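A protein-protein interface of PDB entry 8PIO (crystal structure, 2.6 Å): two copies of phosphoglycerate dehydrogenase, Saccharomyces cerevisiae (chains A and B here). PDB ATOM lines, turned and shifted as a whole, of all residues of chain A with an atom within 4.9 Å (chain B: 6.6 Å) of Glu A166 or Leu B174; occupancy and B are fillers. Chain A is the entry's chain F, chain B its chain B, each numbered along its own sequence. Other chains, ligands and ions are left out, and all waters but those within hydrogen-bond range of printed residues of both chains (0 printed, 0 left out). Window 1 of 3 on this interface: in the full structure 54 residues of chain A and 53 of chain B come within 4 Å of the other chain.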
ATOM      1  N   LEU A 162      33.443   1.569 -20.177  1.00  0.00           N
ATOM      2  CA  LEU A 162      32.054   1.736 -20.659  1.00  0.00           C
ATOM      3  C   LEU A 162      31.350   2.790 -19.810  1.00  0.00           C
ATOM      4  O   LEU A 162      30.673   3.654 -20.390  1.00  0.00           O
ATOM      5  CB  LEU A 162      31.304   0.415 -20.586  1.00  0.00           C
ATOM      6  CG  LEU A 162      29.812   0.522 -20.879  1.00  0.00           C
ATOM      7  CD1 LEU A 162      29.578   0.769 -22.356  1.00  0.00           C
ATOM      8  CD2 LEU A 162      29.069  -0.721 -20.410  1.00  0.00           C
ATOM      9  N   VAL A 163      31.504   2.718 -18.488  1.00  0.00           N
ATOM     10  CA  VAL A 163      30.763   3.585 -17.525  1.00  0.00           C
ATOM     11  C   VAL A 163      31.252   5.034 -17.670  1.00  0.00           C
ATOM     12  O   VAL A 163      30.400   5.941 -17.674  1.00  0.00           O
ATOM     13  CB  VAL A 163      30.879   3.073 -16.082  1.00  0.00           C
ATOM     14  CG1 VAL A 163      30.429   4.125 -15.072  1.00  0.00           C
ATOM     15  CG2 VAL A 163      30.099   1.779 -15.899  1.00  0.00           C
ATOM     16  N   ILE A 164      32.560   5.247 -17.796  1.00  0.00           N
ATOM     17  CA  ILE A 164      33.135   6.604 -18.048  1.00  0.00           C
ATOM     18  C   ILE A 164      32.461   7.157 -19.299  1.00  0.00           C
ATOM     19  O   ILE A 164      31.885   8.251 -19.227  1.00  0.00           O
ATOM     20  CB  ILE A 164      34.667   6.561 -18.190  1.00  0.00           C
ATOM     21  CG1 ILE A 164      35.336   6.111 -16.896  1.00  0.00           C
ATOM     22  CG2 ILE A 164      35.201   7.907 -18.656  1.00  0.00           C
ATOM     23  CD1 ILE A 164      35.148   7.073 -15.740  1.00  0.00           C
ATOM     24  N   GLY A 165      32.516   6.401 -20.395  1.00  0.00           N
ATOM     25  CA  GLY A 165      31.855   6.735 -21.666  1.00  0.00           C
ATOM     26  C   GLY A 165      30.400   7.105 -21.459  1.00  0.00           C
ATOM     27  O   GLY A 165      29.985   8.154 -21.967  1.00  0.00           O
ATOM     28  N   GLU A 166      29.656   6.274 -20.730  1.00  0.00           N
ATOM     29  CA  GLU A 166      28.195   6.433 -20.513  1.00  0.00           C
ATOM     30  C   GLU A 166      27.941   7.666 -19.638  1.00  0.00           C
ATOM     31  O   GLU A 166      26.970   8.381 -19.917  1.00  0.00           O
ATOM     32  CB  GLU A 166      27.596   5.144 -19.942  1.00  0.00           C
ATOM     33  CG  GLU A 166      27.399   4.065 -21.007  1.00  0.00           C
ATOM     34  CD  GLU A 166      26.773   2.770 -20.535  1.00  0.00           C
ATOM     35  OE1 GLU A 166      26.887   2.463 -19.319  1.00  0.00           O
ATOM     36  OE2 GLU A 166      26.161   2.054 -21.391  1.00  0.00           O
ATOM     37  N   ILE A 167      28.793   7.922 -18.645  1.00  0.00           N
ATOM     38  CA  ILE A 167      28.680   9.119 -17.756  1.00  0.00           C
ATOM     39  C   ILE A 167      28.728  10.372 -18.638  1.00  0.00           C
ATOM     40  O   ILE A 167      27.786  11.194 -18.561  1.00  0.00           O
ATOM     41  CB  ILE A 167      29.774   9.130 -16.668  1.00  0.00           C
ATOM     42  CG1 ILE A 167      29.550   8.030 -15.630  1.00  0.00           C
ATOM     43  CG2 ILE A 167      29.876  10.512 -16.010  1.00  0.00           C
ATOM     44  CD1 ILE A 167      30.751   7.762 -14.756  1.00  0.00           C
ATOM     45  N   ILE A 168      29.772  10.498 -19.451  1.00  0.00           N
ATOM     46  CA  ILE A 168      29.988  11.658 -20.369  1.00  0.00           C
ATOM     47  C   ILE A 168      28.807  11.736 -21.347  1.00  0.00           C
ATOM     48  O   ILE A 168      28.281  12.851 -21.559  1.00  0.00           O
ATOM     49  CB  ILE A 168      31.338  11.533 -21.109  1.00  0.00           C
ATOM     50  CG1 ILE A 168      32.524  11.592 -20.151  1.00  0.00           C
ATOM     51  CG2 ILE A 168      31.453  12.583 -22.202  1.00  0.00           C
ATOM     52  CD1 ILE A 168      33.770  10.922 -20.690  1.00  0.00           C
ATOM     53  N   SER A 169      28.411  10.596 -21.918  1.00  0.00           N
ATOM     54  CA  SER A 169      27.360  10.494 -22.956  1.00  0.00           C
ATOM     55  C   SER A 169      26.036  11.032 -22.404  1.00  0.00           C
ATOM     56  O   SER A 169      25.401  11.849 -23.089  1.00  0.00           O
ATOM     57  CB  SER A 169      27.218   9.094 -23.454  1.00  0.00           C
ATOM     58  OG  SER A 169      26.190   9.014 -24.440  1.00  0.00           O
ATOM     59  N   LEU A 170      25.648  10.585 -21.210  1.00  0.00           N
ATOM     60  CA  LEU A 170      24.402  11.012 -20.517  1.00  0.00           C
ATOM     61  C   LEU A 170      24.513  12.487 -20.132  1.00  0.00           C
ATOM     62  O   LEU A 170      23.537  13.229 -20.324  1.00  0.00           O
ATOM     63  CB  LEU A 170      24.199  10.147 -19.271  1.00  0.00           C
ATOM     64  CG  LEU A 170      23.828   8.693 -19.526  1.00  0.00           C
ATOM     65  CD1 LEU A 170      23.830   7.910 -18.221  1.00  0.00           C
ATOM     66  CD2 LEU A 170      22.476   8.589 -20.216  1.00  0.00           C
ATOM     67  N   ALA A 171      25.659  12.874 -19.591  1.00  0.00           N
ATOM     68  CA  ALA A 171      25.981  14.249 -19.148  1.00  0.00           C
ATOM     69  C   ALA A 171      25.742  15.244 -20.293  1.00  0.00           C
ATOM     70  O   ALA A 171      25.364  16.392 -20.004  1.00  0.00           O
ATOM     71  CB  ALA A 171      27.408  14.308 -18.669  1.00  0.00           C
ATOM     72  N   ILE A 283      23.159   4.356 -13.719  1.00  0.00           N
ATOM     73  CA  ILE A 283      23.945   3.464 -14.614  1.00  0.00           C
ATOM     74  C   ILE A 283      24.006   2.086 -13.983  1.00  0.00           C
ATOM     75  O   ILE A 283      24.517   1.980 -12.861  1.00  0.00           O
ATOM     76  CB  ILE A 283      25.348   4.046 -14.869  1.00  0.00           C
ATOM     77  CG1 ILE A 283      25.266   5.430 -15.508  1.00  0.00           C
ATOM     78  CG2 ILE A 283      26.190   3.092 -15.706  1.00  0.00           C
ATOM     79  CD1 ILE A 283      26.601   6.094 -15.693  1.00  0.00           C
ATOM     80  N   ALA A 309      21.624   4.495 -18.215  1.00  0.00           N
ATOM     81  CA  ALA A 309      22.285   3.549 -19.134  1.00  0.00           C
ATOM     82  C   ALA A 309      22.234   2.149 -18.526  1.00  0.00           C
ATOM     83  O   ALA A 309      22.849   1.951 -17.455  1.00  0.00           O
ATOM     84  CB  ALA A 309      23.701   3.991 -19.404  1.00  0.00           C
ATOM     85  N   ILE A 343      20.391   5.239 -22.499  1.00  0.00           N
ATOM     86  CA  ILE A 343      21.326   4.368 -23.276  1.00  0.00           C
ATOM     87  C   ILE A 343      21.029   2.910 -22.920  1.00  0.00           C
ATOM     88  O   ILE A 343      21.096   2.576 -21.743  1.00  0.00           O
ATOM     89  CB  ILE A 343      22.795   4.742 -22.988  1.00  0.00           C
ATOM     90  CG1 ILE A 343      23.090   6.196 -23.365  1.00  0.00           C
ATOM     91  CG2 ILE A 343      23.754   3.779 -23.674  1.00  0.00           C
ATOM     92  CD1 ILE A 343      24.311   6.767 -22.681  1.00  0.00           C
ATOM     93  N   THR A 345      22.076  -1.127 -23.895  1.00  0.00           N
ATOM     94  CA  THR A 345      23.137  -1.974 -24.493  1.00  0.00           C
ATOM     95  C   THR A 345      22.845  -3.437 -24.198  1.00  0.00           C
ATOM     96  O   THR A 345      22.351  -3.781 -23.128  1.00  0.00           O
ATOM     97  CB  THR A 345      24.525  -1.544 -24.009  1.00  0.00           C
ATOM     98  OG1 THR A 345      24.467  -1.322 -22.597  1.00  0.00           O
ATOM     99  CG2 THR A 345      25.016  -0.296 -24.710  1.00  0.00           C
ATOM    100  N   ILE A 348      27.094  -5.767 -23.060  1.00  0.00           N
ATOM    101  CA  ILE A 348      28.398  -5.642 -23.796  1.00  0.00           C
ATOM    102  C   ILE A 348      29.492  -5.158 -22.847  1.00  0.00           C
ATOM    103  O   ILE A 348      30.614  -4.909 -23.334  1.00  0.00           O
ATOM    104  CB  ILE A 348      28.258  -4.695 -24.995  1.00  0.00           C
ATOM    105  CG1 ILE A 348      27.688  -3.336 -24.568  1.00  0.00           C
ATOM    106  CG2 ILE A 348      27.425  -5.344 -26.087  1.00  0.00           C
ATOM    107  CD1 ILE A 348      27.893  -2.243 -25.561  1.00  0.00           C
ATOM    108  N   GLY B 165      34.584  10.830 -24.252  1.00  0.00           N
ATOM    109  CA  GLY B 165      33.283  10.164 -24.442  1.00  0.00           C
ATOM    110  C   GLY B 165      33.182   9.522 -25.813  1.00  0.00           C
ATOM    111  O   GLY B 165      32.818   8.331 -25.887  1.00  0.00           O
ATOM    112  N   ILE B 168      35.629   6.422 -26.462  1.00  0.00           N
ATOM    113  CA  ILE B 168      35.074   5.206 -25.803  1.00  0.00           C
ATOM    114  C   ILE B 168      33.869   4.718 -26.609  1.00  0.00           C
ATOM    115  O   ILE B 168      33.779   3.488 -26.869  1.00  0.00           O
ATOM    116  CB  ILE B 168      34.713   5.498 -24.327  1.00  0.00           C
ATOM    117  CG1 ILE B 168      35.967   5.813 -23.500  1.00  0.00           C
ATOM    118  CG2 ILE B 168      33.920   4.350 -23.723  1.00  0.00           C
ATOM    119  CD1 ILE B 168      35.702   6.611 -22.255  1.00  0.00           C
ATOM    120  N   SER B 169      32.988   5.635 -26.991  1.00  0.00           N
ATOM    121  CA  SER B 169      31.714   5.340 -27.689  1.00  0.00           C
ATOM    122  C   SER B 169      32.005   4.639 -29.020  1.00  0.00           C
ATOM    123  O   SER B 169      31.372   3.610 -29.290  1.00  0.00           O
ATOM    124  CB  SER B 169      30.906   6.585 -27.886  1.00  0.00           C
ATOM    125  OG  SER B 169      29.716   6.303 -28.601  1.00  0.00           O
ATOM    126  N   LEU B 170      32.936   5.182 -29.809  1.00  0.00           N
ATOM    127  CA  LEU B 170      33.358   4.620 -31.128  1.00  0.00           C
ATOM    128  C   LEU B 170      34.065   3.280 -30.909  1.00  0.00           C
ATOM    129  O   LEU B 170      33.781   2.322 -31.658  1.00  0.00           O
ATOM    130  CB  LEU B 170      34.284   5.617 -31.823  1.00  0.00           C
ATOM    131  CG  LEU B 170      33.615   6.897 -32.321  1.00  0.00           C
ATOM    132  CD1 LEU B 170      34.653   7.887 -32.820  1.00  0.00           C
ATOM    133  CD2 LEU B 170      32.586   6.595 -33.413  1.00  0.00           C
ATOM    134  N   ALA B 171      34.949   3.231 -29.921  1.00  0.00           N
ATOM    135  CA  ALA B 171      35.746   2.049 -29.542  1.00  0.00           C
ATOM    136  C   ALA B 171      34.826   0.854 -29.271  1.00  0.00           C
ATOM    137  O   ALA B 171      35.256  -0.295 -29.521  1.00  0.00           O
ATOM    138  CB  ALA B 171      36.580   2.377 -28.335  1.00  0.00           C
ATOM    139  N   ARG B 172      33.612   1.119 -28.771  1.00  0.00           N
ATOM    140  CA  ARG B 172      32.663   0.079 -28.276  1.00  0.00           C
ATOM    141  C   ARG B 172      31.406   0.049 -29.138  1.00  0.00           C
ATOM    142  O   ARG B 172      30.609  -0.891 -28.968  1.00  0.00           O
ATOM    143  CB  ARG B 172      32.302   0.359 -26.814  1.00  0.00           C
ATOM    144  CG  ARG B 172      33.499   0.369 -25.877  1.00  0.00           C
ATOM    145  CD  ARG B 172      34.083  -1.011 -25.711  1.00  0.00           C
ATOM    146  NE  ARG B 172      33.256  -1.817 -24.828  1.00  0.00           N
ATOM    147  CZ  ARG B 172      33.350  -1.816 -23.503  1.00  0.00           C
ATOM    148  NH1 ARG B 172      34.250  -1.053 -22.901  1.00  0.00           N
ATOM    149  NH2 ARG B 172      32.547  -2.579 -22.785  1.00  0.00           N
ATOM    150  N   GLN B 173      31.233   1.045 -30.010  1.00  0.00           N
ATOM    151  CA  GLN B 173      30.048   1.195 -30.902  1.00  0.00           C
ATOM    152  C   GLN B 173      28.776   1.332 -30.044  1.00  0.00           C
ATOM    153  O   GLN B 173      27.794   0.647 -30.352  1.00  0.00           O
ATOM    154  CB  GLN B 173      29.926  -0.008 -31.849  1.00  0.00           C
ATOM    155  CG  GLN B 173      31.185  -0.283 -32.668  1.00  0.00           C
ATOM    156  CD  GLN B 173      31.077  -1.568 -33.462  1.00  0.00           C
ATOM    157  OE1 GLN B 173      29.983  -2.057 -33.754  1.00  0.00           O
ATOM    158  NE2 GLN B 173      32.220  -2.126 -33.826  1.00  0.00           N
ATOM    159  N   LEU B 174      28.809   2.185 -29.008  1.00  0.00           N
ATOM    160  CA  LEU B 174      27.656   2.446 -28.105  1.00  0.00           C
ATOM    161  C   LEU B 174      26.458   2.915 -28.920  1.00  0.00           C
ATOM    162  O   LEU B 174      25.396   2.290 -28.810  1.00  0.00           O
ATOM    163  CB  LEU B 174      28.034   3.511 -27.073  1.00  0.00           C
ATOM    164  CG  LEU B 174      28.795   3.025 -25.853  1.00  0.00           C
ATOM    165  CD1 LEU B 174      28.651   4.023 -24.711  1.00  0.00           C
ATOM    166  CD2 LEU B 174      28.313   1.652 -25.413  1.00  0.00           C
ATOM    167  N   GLY B 175      26.625   4.006 -29.671  1.00  0.00           N
ATOM    168  CA  GLY B 175      25.582   4.584 -30.533  1.00  0.00           C
ATOM    169  C   GLY B 175      24.798   3.499 -31.247  1.00  0.00           C
ATOM    170  O   GLY B 175      23.569   3.449 -31.076  1.00  0.00           O
ATOM    171  N   ASP B 176      25.499   2.648 -31.998  1.00  0.00           N
ATOM    172  CA  ASP B 176      24.908   1.547 -32.809  1.00  0.00           C
ATOM    173  C   ASP B 176      24.129   0.603 -31.885  1.00  0.00           C
ATOM    174  O   ASP B 176      22.943   0.354 -32.161  1.00  0.00           O
ATOM    175  CB  ASP B 176      25.987   0.788 -33.592  1.00  0.00           C
ATOM    176  CG  ASP B 176      26.608   1.583 -34.743  1.00  0.00           C
ATOM    177  OD1 ASP B 176      25.998   2.596 -35.160  1.00  0.00           O
ATOM    178  OD2 ASP B 176      27.701   1.179 -35.217  1.00  0.00           O
ATOM    179  N   ARG B 177      24.785   0.105 -30.834  1.00  0.00           N
ATOM    180  CA  ARG B 177      24.216  -0.863 -29.853  1.00  0.00           C
ATOM    181  C   ARG B 177      22.887  -0.334 -29.310  1.00  0.00           C
ATOM    182  O   ARG B 177      21.916  -1.102 -29.288  1.00  0.00           O
ATOM    183  CB  ARG B 177      25.183  -1.091 -28.693  1.00  0.00           C
ATOM    184  CG  ARG B 177      26.420  -1.892 -29.054  1.00  0.00           C
ATOM    185  CD  ARG B 177      26.081  -3.262 -29.604  1.00  0.00           C
ATOM    186  NE  ARG B 177      25.972  -3.229 -31.044  1.00  0.00           N
ATOM    187  CZ  ARG B 177      27.003  -3.227 -31.875  1.00  0.00           C
ATOM    188  NH1 ARG B 177      26.797  -3.181 -33.178  1.00  0.00           N
ATOM    189  NH2 ARG B 177      28.239  -3.260 -31.403  1.00  0.00           N
ATOM    190  N   SER B 178      22.862   0.927 -28.882  1.00  0.00           N
ATOM    191  CA  SER B 178      21.700   1.583 -28.226  1.00  0.00           C
ATOM    192  C   SER B 178      20.574   1.793 -29.242  1.00  0.00           C
ATOM    193  O   SER B 178      19.398   1.663 -28.857  1.00  0.00           O
ATOM    194  CB  SER B 178      22.099   2.870 -27.582  1.00  0.00           C
ATOM    195  OG  SER B 178      21.027   3.407 -26.828  1.00  0.00           O
ATOM    196  N   ILE B 179      20.928   2.106 -30.484  1.00  0.00           N
ATOM    197  CA  ILE B 179      19.964   2.303 -31.608  1.00  0.00           C
ATOM    198  C   ILE B 179      19.312   0.950 -31.933  1.00  0.00           C
ATOM    199  O   ILE B 179      18.086   0.912 -32.089  1.00  0.00           O
ATOM    200  CB  ILE B 179      20.658   2.937 -32.831  1.00  0.00           C
ATOM    201  CG1 ILE B 179      20.754   4.460 -32.686  1.00  0.00           C
ATOM    202  CG2 ILE B 179      19.956   2.540 -34.123  1.00  0.00           C
ATOM    203  CD1 ILE B 179      21.792   5.103 -33.573  1.00  0.00           C
ATOM    204  N   ASN B 341      28.438   3.423 -37.105  1.00  0.00           N
ATOM    205  CA  ASN B 341      29.472   3.851 -36.117  1.00  0.00           C
ATOM    206  C   ASN B 341      29.973   5.256 -36.461  1.00  0.00           C
ATOM    207  O   ASN B 341      31.181   5.512 -36.287  1.00  0.00           O
ATOM    208  CB  ASN B 341      30.641   2.862 -36.025  1.00  0.00           C
ATOM    209  CG  ASN B 341      31.357   2.927 -34.685  1.00  0.00           C
ATOM    210  OD1 ASN B 341      30.753   3.263 -33.673  1.00  0.00           O
ATOM    211  ND2 ASN B 341      32.638   2.608 -34.667  1.00  0.00           N
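NH2 of Arg B172 is in hydrogen-bond range of O of Ile A348, 3.1 Å away.
The backbone NH (N) of Leu B174 lies within hydrogen-bond range of the backbone carbonyl oxygen (O) of Ser B169. NH2 of Arg B177 is in hydrogen-bond range of OE1 of Gln B173 (3.2 Å).
Among the printed residues, merely in contact across the chains: Leu A162 with Leu B174 (3.4 Å), Ile A168 with Gly B165 (3.7 Å), Ile A343 with Ser B178 (3.7 Å), Gly A165 with Ile B168 (3.7 Å), Ile A348 with Arg B177 (3.8 Å), Ile A164 with Ile B168 (3.9 Å), Leu A162 with Arg B172 (3.9 Å), Thr A345 with Leu B174 (3.9 Å), Glu A166 with Leu B174 (3.9 Å) and Ile A348 with Leu B174 (3.9 Å).
Glu A166 touches one residue of chain B. Leu B174 touches just these residues of chain A: Leu A162, Glu A166, Thr A345 and Ile A348. Of the printed residues of chain B, Gly A165 touches Ile B168. Of the printed residues of chain A, Ile B168 touches Ile A164 (3.9 Å) and Gly A165 (3.7 Å). Of the printed residues of chain A, Arg B177 touches Ile A348 (3.8 Å). Printed residues of chain B within 4 Å of Ile A164: Ile B168. Of the printed residues of chain B, Ile A168 touches Gly B165. Asp B176 touches none of the printed residues of chain A. The nearest residue of chain B that does not touch Glu A166 is Ile B168 (5.6 Å).
Hydrophobic or aromatic side chains of chain B within 4 Å of the printed part of chain A: Ile B168 and Leu B174. Printed residues of chain A that touch a printed residue of chain B: Leu A162, Ile A164, Gly A165, Glu A166, Ile A168, Ile A343, Thr A345 and Ile A348. Hydrophobic or aromatic side chains of chain A that line the printed part of chain B: Leu A162, Ile A164, Ile A168 and Ile A348. Among the printed residues, 11 pairs touch across the chains. Among the printed residues, no Asp or Glu carboxylate lies within 4 Å of a Lys or Arg side-chain nitrogen of the other chain.
Gly A165 touches Ile B168, and with the chains exchanged Ile A168 touches Gly B165. Of the 11 pairs that touch across the chains among the printed residues, 2 have their exchanged pair printed and touching as well.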
